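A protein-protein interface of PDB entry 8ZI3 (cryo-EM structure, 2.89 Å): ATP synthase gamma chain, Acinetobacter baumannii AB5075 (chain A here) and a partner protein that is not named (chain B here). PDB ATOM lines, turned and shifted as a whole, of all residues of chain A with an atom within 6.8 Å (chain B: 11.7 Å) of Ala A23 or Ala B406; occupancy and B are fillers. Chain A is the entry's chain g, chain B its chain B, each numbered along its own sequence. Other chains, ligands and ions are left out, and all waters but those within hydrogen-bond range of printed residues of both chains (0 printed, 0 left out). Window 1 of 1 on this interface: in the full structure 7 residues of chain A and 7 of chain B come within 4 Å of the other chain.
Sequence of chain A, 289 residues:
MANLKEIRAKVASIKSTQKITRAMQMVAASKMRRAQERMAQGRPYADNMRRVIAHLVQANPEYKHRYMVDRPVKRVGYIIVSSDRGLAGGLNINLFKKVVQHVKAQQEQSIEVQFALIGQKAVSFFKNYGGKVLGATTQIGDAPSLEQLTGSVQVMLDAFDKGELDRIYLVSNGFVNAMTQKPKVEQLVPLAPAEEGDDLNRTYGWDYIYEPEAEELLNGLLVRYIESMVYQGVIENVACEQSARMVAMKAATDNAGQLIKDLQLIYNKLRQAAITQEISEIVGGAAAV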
ATOM      1  N   SER A  16     -12.409  27.918  40.073  1.00  0.00           N
ATOM      2  CA  SER A  16     -13.059  26.949  39.193  1.00  0.00           C
ATOM      3  C   SER A  16     -14.438  27.434  38.761  1.00  0.00           C
ATOM      4  O   SER A  16     -14.821  27.291  37.589  1.00  0.00           O
ATOM      5  CB  SER A  16     -13.161  25.594  39.891  1.00  0.00           C
ATOM      6  OG  SER A  16     -13.760  25.726  41.169  1.00  0.00           O
ATOM      7  N   GLN A  18     -15.381  30.531  38.488  1.00  0.00           N
ATOM      8  CA  GLN A  18     -15.144  31.592  37.518  1.00  0.00           C
ATOM      9  C   GLN A  18     -14.879  31.019  36.131  1.00  0.00           C
ATOM     10  O   GLN A  18     -15.433  31.499  35.133  1.00  0.00           O
ATOM     11  CB  GLN A  18     -13.967  32.453  37.981  1.00  0.00           C
ATOM     12  CG  GLN A  18     -13.833  33.784  37.272  1.00  0.00           C
ATOM     13  CD  GLN A  18     -12.663  34.595  37.792  1.00  0.00           C
ATOM     14  OE1 GLN A  18     -11.717  34.047  38.356  1.00  0.00           O
ATOM     15  NE2 GLN A  18     -12.722  35.907  37.604  1.00  0.00           N
ATOM     16  N   LYS A  19     -14.044  29.980  36.052  1.00  0.00           N
ATOM     17  CA  LYS A  19     -13.731  29.380  34.756  1.00  0.00           C
ATOM     18  C   LYS A  19     -14.980  28.798  34.098  1.00  0.00           C
ATOM     19  O   LYS A  19     -15.242  29.032  32.907  1.00  0.00           O
ATOM     20  CB  LYS A  19     -12.660  28.304  34.923  1.00  0.00           C
ATOM     21  CG  LYS A  19     -11.350  28.813  35.495  1.00  0.00           C
ATOM     22  CD  LYS A  19     -10.290  27.723  35.510  1.00  0.00           C
ATOM     23  CE  LYS A  19      -9.650  27.556  34.144  1.00  0.00           C
ATOM     24  NZ  LYS A  19      -8.819  26.322  34.068  1.00  0.00           N
ATOM     25  N   ILE A  20     -15.770  28.037  34.863  1.00  0.00           N
ATOM     26  CA  ILE A  20     -16.955  27.418  34.271  1.00  0.00           C
ATOM     27  C   ILE A  20     -17.967  28.479  33.850  1.00  0.00           C
ATOM     28  O   ILE A  20     -18.658  28.322  32.832  1.00  0.00           O
ATOM     29  CB  ILE A  20     -17.573  26.373  35.222  1.00  0.00           C
ATOM     30  CG1 ILE A  20     -18.302  27.036  36.392  1.00  0.00           C
ATOM     31  CG2 ILE A  20     -16.513  25.401  35.716  1.00  0.00           C
ATOM     32  CD1 ILE A  20     -19.257  26.115  37.118  1.00  0.00           C
ATOM     33  N   THR A  21     -18.065  29.581  34.598  1.00  0.00           N
ATOM     34  CA  THR A  21     -19.023  30.616  34.230  1.00  0.00           C
ATOM     35  C   THR A  21     -18.568  31.359  32.974  1.00  0.00           C
ATOM     36  O   THR A  21     -19.395  31.733  32.133  1.00  0.00           O
ATOM     37  CB  THR A  21     -19.231  31.565  35.412  1.00  0.00           C
ATOM     38  OG1 THR A  21     -20.164  30.973  36.325  1.00  0.00           O
ATOM     39  CG2 THR A  21     -19.823  32.864  34.949  1.00  0.00           C
ATOM     40  N   ARG A  22     -17.254  31.549  32.805  1.00  0.00           N
ATOM     41  CA  ARG A  22     -16.752  32.072  31.533  1.00  0.00           C
ATOM     42  C   ARG A  22     -17.127  31.152  30.376  1.00  0.00           C
ATOM     43  O   ARG A  22     -17.558  31.617  29.307  1.00  0.00           O
ATOM     44  CB  ARG A  22     -15.233  32.247  31.586  1.00  0.00           C
ATOM     45  CG  ARG A  22     -14.728  33.231  32.619  1.00  0.00           C
ATOM     46  CD  ARG A  22     -13.207  33.284  32.637  1.00  0.00           C
ATOM     47  NE  ARG A  22     -12.666  34.093  31.552  1.00  0.00           N
ATOM     48  CZ  ARG A  22     -12.233  33.605  30.396  1.00  0.00           C
ATOM     49  NH1 ARG A  22     -12.263  32.308  30.138  1.00  0.00           N
ATOM     50  NH2 ARG A  22     -11.755  34.440  29.477  1.00  0.00           N
ATOM     51  N   ALA A  23     -16.954  29.842  30.568  1.00  0.00           N
ATOM     52  CA  ALA A  23     -17.323  28.894  29.520  1.00  0.00           C
ATOM     53  C   ALA A  23     -18.799  29.027  29.161  1.00  0.00           C
ATOM     54  O   ALA A  23     -19.172  29.025  27.979  1.00  0.00           O
ATOM     55  CB  ALA A  23     -17.000  27.469  29.967  1.00  0.00           C
ATOM     56  N   MET A  24     -19.655  29.150  30.179  1.00  0.00           N
ATOM     57  CA  MET A  24     -21.080  29.334  29.924  1.00  0.00           C
ATOM     58  C   MET A  24     -21.359  30.637  29.184  1.00  0.00           C
ATOM     59  O   MET A  24     -22.269  30.689  28.349  1.00  0.00           O
ATOM     60  CB  MET A  24     -21.866  29.292  31.232  1.00  0.00           C
ATOM     61  CG  MET A  24     -21.881  27.929  31.894  1.00  0.00           C
ATOM     62  SD  MET A  24     -22.740  27.938  33.474  1.00  0.00           S
ATOM     63  CE  MET A  24     -24.439  28.106  32.929  1.00  0.00           C
ATOM     64  N   GLN A  25     -20.602  31.693  29.479  1.00  0.00           N
ATOM     65  CA  GLN A  25     -20.777  32.954  28.760  1.00  0.00           C
ATOM     66  C   GLN A  25     -20.488  32.783  27.272  1.00  0.00           C
ATOM     67  O   GLN A  25     -21.249  33.257  26.417  1.00  0.00           O
ATOM     68  CB  GLN A  25     -19.877  34.028  29.370  1.00  0.00           C
ATOM     69  CG  GLN A  25     -19.931  35.370  28.661  1.00  0.00           C
ATOM     70  CD  GLN A  25     -18.931  36.364  29.222  1.00  0.00           C
ATOM     71  OE1 GLN A  25     -18.969  37.552  28.898  1.00  0.00           O
ATOM     72  NE2 GLN A  25     -18.029  35.882  30.068  1.00  0.00           N
ATOM     73  N   MET A  26     -19.391  32.096  26.940  1.00  0.00           N
ATOM     74  CA  MET A  26     -19.090  31.850  25.527  1.00  0.00           C
ATOM     75  C   MET A  26     -20.162  30.987  24.862  1.00  0.00           C
ATOM     76  O   MET A  26     -20.548  31.233  23.705  1.00  0.00           O
ATOM     77  CB  MET A  26     -17.711  31.207  25.373  1.00  0.00           C
ATOM     78  CG  MET A  26     -16.550  32.074  25.847  1.00  0.00           C
ATOM     79  SD  MET A  26     -16.296  33.605  24.935  1.00  0.00           S
ATOM     80  CE  MET A  26     -14.881  34.284  25.799  1.00  0.00           C
ATOM     81  N   VAL A  27     -20.648  29.965  25.572  1.00  0.00           N
ATOM     82  CA  VAL A  27     -21.706  29.117  25.025  1.00  0.00           C
ATOM     83  C   VAL A  27     -22.946  29.950  24.720  1.00  0.00           C
ATOM     84  O   VAL A  27     -23.577  29.807  23.662  1.00  0.00           O
ATOM     85  CB  VAL A  27     -22.024  27.966  25.997  1.00  0.00           C
ATOM     86  CG1 VAL A  27     -23.337  27.297  25.625  1.00  0.00           C
ATOM     87  CG2 VAL A  27     -20.891  26.958  26.005  1.00  0.00           C
ATOM     88  N   ALA A  28     -23.311  30.836  25.649  1.00  0.00           N
ATOM     89  CA  ALA A  28     -24.455  31.712  25.433  1.00  0.00           C
ATOM     90  C   ALA A  28     -24.226  32.630  24.240  1.00  0.00           C
ATOM     91  O   ALA A  28     -25.165  32.931  23.498  1.00  0.00           O
ATOM     92  CB  ALA A  28     -24.737  32.529  26.694  1.00  0.00           C
ATOM     93  N   THR A 253     -18.732  36.374  36.807  1.00  0.00           N
ATOM     94  CA  THR A 253     -17.276  36.294  36.712  1.00  0.00           C
ATOM     95  C   THR A 253     -16.612  37.475  37.408  1.00  0.00           C
ATOM     96  O   THR A 253     -15.654  37.304  38.180  1.00  0.00           O
ATOM     97  CB  THR A 253     -16.834  36.241  35.250  1.00  0.00           C
ATOM     98  OG1 THR A 253     -17.569  37.209  34.490  1.00  0.00           O
ATOM     99  CG2 THR A 253     -17.056  34.871  34.673  1.00  0.00           C
ATOM    100  N   LEU B 398      -0.391  20.935  23.910  1.00  0.00           N
ATOM    101  CA  LEU B 398      -0.660  20.894  25.343  1.00  0.00           C
ATOM    102  C   LEU B 398      -1.062  22.265  25.869  1.00  0.00           C
ATOM    103  O   LEU B 398      -1.975  22.376  26.694  1.00  0.00           O
ATOM    104  CB  LEU B 398       0.559  20.364  26.097  1.00  0.00           C
ATOM    105  CG  LEU B 398       0.600  18.853  26.330  1.00  0.00           C
ATOM    106  CD1 LEU B 398       1.605  18.506  27.415  1.00  0.00           C
ATOM    107  CD2 LEU B 398      -0.779  18.323  26.685  1.00  0.00           C
ATOM    108  N   ALA B 399      -0.390  23.323  25.406  1.00  0.00           N
ATOM    109  CA  ALA B 399      -0.765  24.667  25.837  1.00  0.00           C
ATOM    110  C   ALA B 399      -2.190  25.007  25.410  1.00  0.00           C
ATOM    111  O   ALA B 399      -2.975  25.547  26.203  1.00  0.00           O
ATOM    112  CB  ALA B 399       0.221  25.692  25.282  1.00  0.00           C
ATOM    113  N   GLN B 400      -2.545  24.686  24.164  1.00  0.00           N
ATOM    114  CA  GLN B 400      -3.893  24.961  23.680  1.00  0.00           C
ATOM    115  C   GLN B 400      -4.940  24.164  24.447  1.00  0.00           C
ATOM    116  O   GLN B 400      -6.025  24.684  24.730  1.00  0.00           O
ATOM    117  CB  GLN B 400      -3.987  24.662  22.185  1.00  0.00           C
ATOM    118  CG  GLN B 400      -3.682  25.856  21.300  1.00  0.00           C
ATOM    119  CD  GLN B 400      -3.306  25.455  19.890  1.00  0.00           C
ATOM    120  OE1 GLN B 400      -3.593  24.340  19.452  1.00  0.00           O
ATOM    121  NE2 GLN B 400      -2.658  26.362  19.170  1.00  0.00           N
ATOM    122  N   TYR B 401      -4.643  22.909  24.786  1.00  0.00           N
ATOM    123  CA  TYR B 401      -5.580  22.129  25.588  1.00  0.00           C
ATOM    124  C   TYR B 401      -5.723  22.698  26.993  1.00  0.00           C
ATOM    125  O   TYR B 401      -6.823  22.696  27.554  1.00  0.00           O
ATOM    126  CB  TYR B 401      -5.141  20.669  25.659  1.00  0.00           C
ATOM    127  CG  TYR B 401      -6.084  19.808  26.465  1.00  0.00           C
ATOM    128  CD1 TYR B 401      -7.399  19.621  26.061  1.00  0.00           C
ATOM    129  CD2 TYR B 401      -5.666  19.193  27.636  1.00  0.00           C
ATOM    130  CE1 TYR B 401      -8.267  18.838  26.796  1.00  0.00           C
ATOM    131  CE2 TYR B 401      -6.527  18.408  28.376  1.00  0.00           C
ATOM    132  CZ  TYR B 401      -7.826  18.235  27.952  1.00  0.00           C
ATOM    133  OH  TYR B 401      -8.686  17.455  28.687  1.00  0.00           O
ATOM    134  N   ARG B 402      -4.625  23.172  27.584  1.00  0.00           N
ATOM    135  CA  ARG B 402      -4.715  23.772  28.910  1.00  0.00           C
ATOM    136  C   ARG B 402      -5.537  25.051  28.896  1.00  0.00           C
ATOM    137  O   ARG B 402      -6.281  25.316  29.847  1.00  0.00           O
ATOM    138  CB  ARG B 402      -3.323  24.064  29.467  1.00  0.00           C
ATOM    139  CG  ARG B 402      -2.526  22.839  29.862  1.00  0.00           C
ATOM    140  CD  ARG B 402      -1.333  23.236  30.710  1.00  0.00           C
ATOM    141  NE  ARG B 402      -0.563  24.313  30.100  1.00  0.00           N
ATOM    142  CZ  ARG B 402       0.378  24.139  29.182  1.00  0.00           C
ATOM    143  NH1 ARG B 402       0.696  22.935  28.737  1.00  0.00           N
ATOM    144  NH2 ARG B 402       1.015  25.201  28.698  1.00  0.00           N
ATOM    145  N   GLU B 403      -5.416  25.859  27.838  1.00  0.00           N
ATOM    146  CA  GLU B 403      -6.067  27.166  27.846  1.00  0.00           C
ATOM    147  C   GLU B 403      -7.587  27.030  27.819  1.00  0.00           C
ATOM    148  O   GLU B 403      -8.297  27.852  28.411  1.00  0.00           O
ATOM    149  CB  GLU B 403      -5.515  28.025  26.694  1.00  0.00           C
ATOM    150  CG  GLU B 403      -6.261  29.323  26.310  1.00  0.00           C
ATOM    151  CD  GLU B 403      -7.601  29.122  25.628  1.00  0.00           C
ATOM    152  OE1 GLU B 403      -7.895  27.990  25.204  1.00  0.00           O
ATOM    153  OE2 GLU B 403      -8.368  30.105  25.522  1.00  0.00           O
ATOM    154  N   LEU B 404      -8.107  26.003  27.147  1.00  0.00           N
ATOM    155  CA  LEU B 404      -9.545  25.725  27.137  1.00  0.00           C
ATOM    156  C   LEU B 404      -9.767  24.277  27.570  1.00  0.00           C
ATOM    157  O   LEU B 404      -9.391  23.339  26.863  1.00  0.00           O
ATOM    158  CB  LEU B 404     -10.163  26.024  25.766  1.00  0.00           C
ATOM    159  CG  LEU B 404      -9.752  25.341  24.455  1.00  0.00           C
ATOM    160  CD1 LEU B 404     -10.589  24.113  24.167  1.00  0.00           C
ATOM    161  CD2 LEU B 404      -9.839  26.316  23.291  1.00  0.00           C
ATOM    162  N   ALA B 405     -10.361  24.097  28.749  1.00  0.00           N
ATOM    163  CA  ALA B 405     -10.632  22.762  29.271  1.00  0.00           C
ATOM    164  C   ALA B 405     -12.064  22.653  29.774  1.00  0.00           C
ATOM    165  O   ALA B 405     -12.632  21.557  29.818  1.00  0.00           O
ATOM    166  CB  ALA B 405      -9.649  22.416  30.390  1.00  0.00           C
ATOM    167  N   ALA B 406     -12.654  23.786  30.164  1.00  0.00           N
ATOM    168  CA  ALA B 406     -14.028  23.773  30.651  1.00  0.00           C
ATOM    169  C   ALA B 406     -15.019  23.457  29.540  1.00  0.00           C
ATOM    170  O   ALA B 406     -16.136  23.006  29.819  1.00  0.00           O
ATOM    171  CB  ALA B 406     -14.369  25.114  31.298  1.00  0.00           C
ATOM    172  N   PHE B 407     -14.636  23.681  28.287  1.00  0.00           N
ATOM    173  CA  PHE B 407     -15.505  23.474  27.129  1.00  0.00           C
ATOM    174  C   PHE B 407     -15.716  22.005  26.788  1.00  0.00           C
ATOM    175  O   PHE B 407     -16.297  21.727  25.731  1.00  0.00           O
ATOM    176  CB  PHE B 407     -14.938  24.206  25.912  1.00  0.00           C
ATOM    177  CG  PHE B 407     -14.866  25.698  26.077  1.00  0.00           C
ATOM    178  CD1 PHE B 407     -13.829  26.285  26.786  1.00  0.00           C
ATOM    179  CD2 PHE B 407     -15.832  26.515  25.517  1.00  0.00           C
ATOM    180  CE1 PHE B 407     -13.762  27.656  26.937  1.00  0.00           C
ATOM    181  CE2 PHE B 407     -15.769  27.888  25.664  1.00  0.00           C
ATOM    182  CZ  PHE B 407     -14.733  28.458  26.375  1.00  0.00           C
ATOM    183  N   ALA B 408     -15.261  21.069  27.625  1.00  0.00           N
ATOM    184  CA  ALA B 408     -15.425  19.653  27.314  1.00  0.00           C
ATOM    185  C   ALA B 408     -16.896  19.254  27.276  1.00  0.00           C
ATOM    186  O   ALA B 408     -17.316  18.483  26.404  1.00  0.00           O
ATOM    187  CB  ALA B 408     -14.665  18.801  28.329  1.00  0.00           C
ATOM    188  N   GLN B 409     -17.696  19.767  28.213  1.00  0.00           N
ATOM    189  CA  GLN B 409     -19.092  19.353  28.307  1.00  0.00           C
ATOM    190  C   GLN B 409     -19.958  19.964  27.212  1.00  0.00           C
ATOM    191  O   GLN B 409     -20.968  19.365  26.828  1.00  0.00           O
ATOM    192  CB  GLN B 409     -19.651  19.710  29.685  1.00  0.00           C
ATOM    193  CG  GLN B 409     -19.426  21.153  30.096  1.00  0.00           C
ATOM    194  CD  GLN B 409     -19.681  21.379  31.573  1.00  0.00           C
ATOM    195  OE1 GLN B 409     -20.125  20.478  32.282  1.00  0.00           O
ATOM    196  NE2 GLN B 409     -19.400  22.588  32.043  1.00  0.00           N
ATOM    197  N   PHE B 410     -19.589  21.134  26.699  1.00  0.00           N
ATOM    198  CA  PHE B 410     -20.336  21.801  25.634  1.00  0.00           C
ATOM    199  C   PHE B 410     -19.704  21.571  24.269  1.00  0.00           C
ATOM    200  O   PHE B 410     -19.709  22.467  23.421  1.00  0.00           O
ATOM    201  CB  PHE B 410     -20.451  23.296  25.918  1.00  0.00           C
ATOM    202  CG  PHE B 410     -20.741  23.624  27.354  1.00  0.00           C
ATOM    203  CD1 PHE B 410     -21.951  23.274  27.927  1.00  0.00           C
ATOM    204  CD2 PHE B 410     -19.807  24.292  28.126  1.00  0.00           C
ATOM    205  CE1 PHE B 410     -22.221  23.579  29.247  1.00  0.00           C
ATOM    206  CE2 PHE B 410     -20.072  24.600  29.446  1.00  0.00           C
ATOM    207  CZ  PHE B 410     -21.281  24.243  30.007  1.00  0.00           C
ATOM    208  N   ALA B 411     -19.164  20.371  24.033  1.00  0.00           N
ATOM    209  CA  ALA B 411     -18.373  20.122  22.831  1.00  0.00           C
ATOM    210  C   ALA B 411     -19.174  20.375  21.559  1.00  0.00           C
ATOM    211  O   ALA B 411     -18.634  20.889  20.571  1.00  0.00           O
ATOM    212  CB  ALA B 411     -17.835  18.692  22.848  1.00  0.00           C
ATOM    213  N   SER B 412     -20.460  20.018  21.558  1.00  0.00           N
ATOM    214  CA  SER B 412     -21.274  20.208  20.362  1.00  0.00           C
ATOM    215  C   SER B 412     -21.474  21.683  20.039  1.00  0.00           C
ATOM    216  O   SER B 412     -21.778  22.031  18.892  1.00  0.00           O
ATOM    217  CB  SER B 412     -22.628  19.520  20.533  1.00  0.00           C
ATOM    218  OG  SER B 412     -23.599  20.425  21.031  1.00  0.00           O
ATOM    219  N   ASP B 413     -21.311  22.562  21.029  1.00  0.00           N
ATOM    220  CA  ASP B 413     -21.602  23.976  20.815  1.00  0.00           C
ATOM    221  C   ASP B 413     -20.526  24.666  19.987  1.00  0.00           C
ATOM    222  O   ASP B 413     -20.845  25.519  19.152  1.00  0.00           O
ATOM    223  CB  ASP B 413     -21.771  24.684  22.157  1.00  0.00           C
ATOM    224  CG  ASP B 413     -22.145  26.141  22.001  1.00  0.00           C
ATOM    225  OD1 ASP B 413     -21.231  26.985  21.889  1.00  0.00           O
ATOM    226  OD2 ASP B 413     -23.356  26.446  21.983  1.00  0.00           O
ATOM    227  N   LEU B 414     -19.257  24.325  20.199  1.00  0.00           N
ATOM    228  CA  LEU B 414     -18.186  25.004  19.488  1.00  0.00           C
ATOM    229  C   LEU B 414     -18.153  24.580  18.022  1.00  0.00           C
ATOM    230  O   LEU B 414     -18.775  23.596  17.612  1.00  0.00           O
ATOM    231  CB  LEU B 414     -16.826  24.729  20.137  1.00  0.00           C
ATOM    232  CG  LEU B 414     -16.645  24.791  21.656  1.00  0.00           C
ATOM    233  CD1 LEU B 414     -17.014  23.476  22.311  1.00  0.00           C
ATOM    234  CD2 LEU B 414     -15.223  25.184  22.019  1.00  0.00           C
ATOM    235  N   ASP B 415     -17.411  25.347  17.226  1.00  0.00           N
ATOM    236  CA  ASP B 415     -17.285  25.084  15.800  1.00  0.00           C
ATOM    237  C   ASP B 415     -16.254  23.978  15.567  1.00  0.00           C
ATOM    238  O   ASP B 415     -15.809  23.299  16.496  1.00  0.00           O
ATOM    239  CB  ASP B 415     -16.940  26.370  15.056  1.00  0.00           C
ATOM    240  CG  ASP B 415     -15.606  26.950  15.476  1.00  0.00           C
ATOM    241  OD1 ASP B 415     -14.561  26.428  15.034  1.00  0.00           O
ATOM    242  OD2 ASP B 415     -15.603  27.930  16.249  1.00  0.00           O
ATOM    243  N   THR B 418     -12.210  24.529  17.051  1.00  0.00           N
ATOM    244  CA  THR B 418     -12.008  24.371  18.486  1.00  0.00           C
ATOM    245  C   THR B 418     -12.286  22.940  18.935  1.00  0.00           C
ATOM    246  O   THR B 418     -11.612  22.425  19.835  1.00  0.00           O
ATOM    247  CB  THR B 418     -12.890  25.361  19.246  1.00  0.00           C
ATOM    248  OG1 THR B 418     -14.189  25.392  18.648  1.00  0.00           O
ATOM    249  CG2 THR B 418     -12.283  26.755  19.199  1.00  0.00           C
ATOM    250  N   ARG B 419     -13.269  22.279  18.321  1.00  0.00           N
ATOM    251  CA  ARG B 419     -13.516  20.877  18.640  1.00  0.00           C
ATOM    252  C   ARG B 419     -12.332  20.005  18.237  1.00  0.00           C
ATOM    253  O   ARG B 419     -11.945  19.092  18.977  1.00  0.00           O
ATOM    254  CB  ARG B 419     -14.797  20.401  17.959  1.00  0.00           C
ATOM    255  CG  ARG B 419     -15.823  19.819  18.918  1.00  0.00           C
ATOM    256  CD  ARG B 419     -17.017  19.238  18.180  1.00  0.00           C
ATOM    257  NE  ARG B 419     -16.626  18.221  17.212  1.00  0.00           N
ATOM    258  CZ  ARG B 419     -16.726  18.362  15.897  1.00  0.00           C
ATOM    259  NH1 ARG B 419     -17.208  19.468  15.355  1.00  0.00           N
ATOM    260  NH2 ARG B 419     -16.332  17.367  15.107  1.00  0.00           N
ATOM    261  N   GLN B 421      -9.259  21.034  18.085  1.00  0.00           N
ATOM    262  CA  GLN B 421      -8.236  21.339  19.079  1.00  0.00           C
ATOM    263  C   GLN B 421      -8.461  20.548  20.361  1.00  0.00           C
ATOM    264  O   GLN B 421      -7.513  20.008  20.941  1.00  0.00           O
ATOM    265  CB  GLN B 421      -8.223  22.839  19.371  1.00  0.00           C
ATOM    266  CG  GLN B 421      -7.728  23.694  18.218  1.00  0.00           C
ATOM    267  CD  GLN B 421      -7.277  25.069  18.663  1.00  0.00           C
ATOM    268  OE1 GLN B 421      -6.392  25.201  19.509  1.00  0.00           O
ATOM    269  NE2 GLN B 421      -7.886  26.104  18.098  1.00  0.00           N
ATOM    270  N   LEU B 422      -9.714  20.466  20.815  1.00  0.00           N
ATOM    271  CA  LEU B 422     -10.029  19.695  22.016  1.00  0.00           C
ATOM    272  C   LEU B 422      -9.675  18.223  21.842  1.00  0.00           C
ATOM    273  O   LEU B 422      -9.056  17.612  22.723  1.00  0.00           O
ATOM    274  CB  LEU B 422     -11.509  19.847  22.364  1.00  0.00           C
ATOM    275  CG  LEU B 422     -11.890  19.633  23.831  1.00  0.00           C
ATOM    276  CD1 LEU B 422     -11.319  20.716  24.722  1.00  0.00           C
ATOM    277  CD2 LEU B 422     -13.402  19.558  23.979  1.00  0.00           C
ATOM    278  N   GLU B 423     -10.072  17.631  20.716  1.00  0.00           N
ATOM    279  CA  GLU B 423      -9.797  16.212  20.506  1.00  0.00           C
ATOM    280  C   GLU B 423      -8.298  15.947  20.398  1.00  0.00           C
ATOM    281  O   GLU B 423      -7.795  14.961  20.953  1.00  0.00           O
ATOM    282  CB  GLU B 423     -10.533  15.706  19.266  1.00  0.00           C
ATOM    283  CG  GLU B 423     -12.020  16.031  19.260  1.00  0.00           C
ATOM    284  CD  GLU B 423     -12.889  14.825  18.966  1.00  0.00           C
ATOM    285  OE1 GLU B 423     -13.699  14.449  19.839  1.00  0.00           O
ATOM    286  OE2 GLU B 423     -12.767  14.256  17.860  1.00  0.00           O
ATOM    287  N   GLN B 426      -6.833  16.086  23.878  1.00  0.00           N
ATOM    288  CA  GLN B 426      -7.139  14.872  24.630  1.00  0.00           C
ATOM    289  C   GLN B 426      -6.240  13.719  24.195  1.00  0.00           C
ATOM    290  O   GLN B 426      -5.689  12.990  25.033  1.00  0.00           O
ATOM    291  CB  GLN B 426      -8.611  14.502  24.451  1.00  0.00           C
ATOM    292  CG  GLN B 426      -9.579  15.462  25.117  1.00  0.00           C
ATOM    293  CD  GLN B 426     -11.017  14.994  25.022  1.00  0.00           C
ATOM    294  OE1 GLN B 426     -11.284  13.823  24.757  1.00  0.00           O
ATOM    295  NE2 GLN B 426     -11.952  15.911  25.236  1.00  0.00           N
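Of chain B, only Ala B406 (3.8 Å) comes within 4 Å of Ala A23.
Ala B406 touches just one residue of chain A: Ala A23.
Lys A19 touches none of the printed residues of chain B.
No residue of chain B comes within 4 Å of Ile A20.
No residue of chain B comes within 4 Å of Thr A21.
No residue of chain B comes within 4 Å of Arg A22.
No residue of chain B comes within 4 Å of Met A24.
Of chain B, only Phe B407 comes within 4 Å of Met A26.
Val A27 touches just these residues of chain B: Phe B410 and Asp B413.
Printed residues of chain A within 4 Å of Phe B410: Val A27 (3.6 Å).
Of the printed residues of chain A, Phe B407 touches Met A26.
Of the printed residues of chain A, Asp B413 touches Val A27.
The nearest residue of chain B that does not touch Ala A23 is Phe B407 (4.1 Å).
Hydrophobic or aromatic side chains of chain B within 4 Å of the printed part of chain A: Ala B406, Phe B407 and Phe B410.
Along chain B the printed residues that touch a printed residue of chain A span positions 406 to 413.
Of the 13 printed residues of chain A, 3 touch a printed residue of chain B.
Among the printed residues, no Asp or Glu carboxylate lies within 4 Å of a Lys or Arg side-chain nitrogen of the other chain.
Among the printed residues, pairs that only touch across the chains: Val A27 with Phe B410 (3.6 Å), Val A27 with Asp B413 (3.7 Å), Ala A23 with Ala B406 (3.8 Å) and Met A26 with Phe B407 (3.9 Å).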
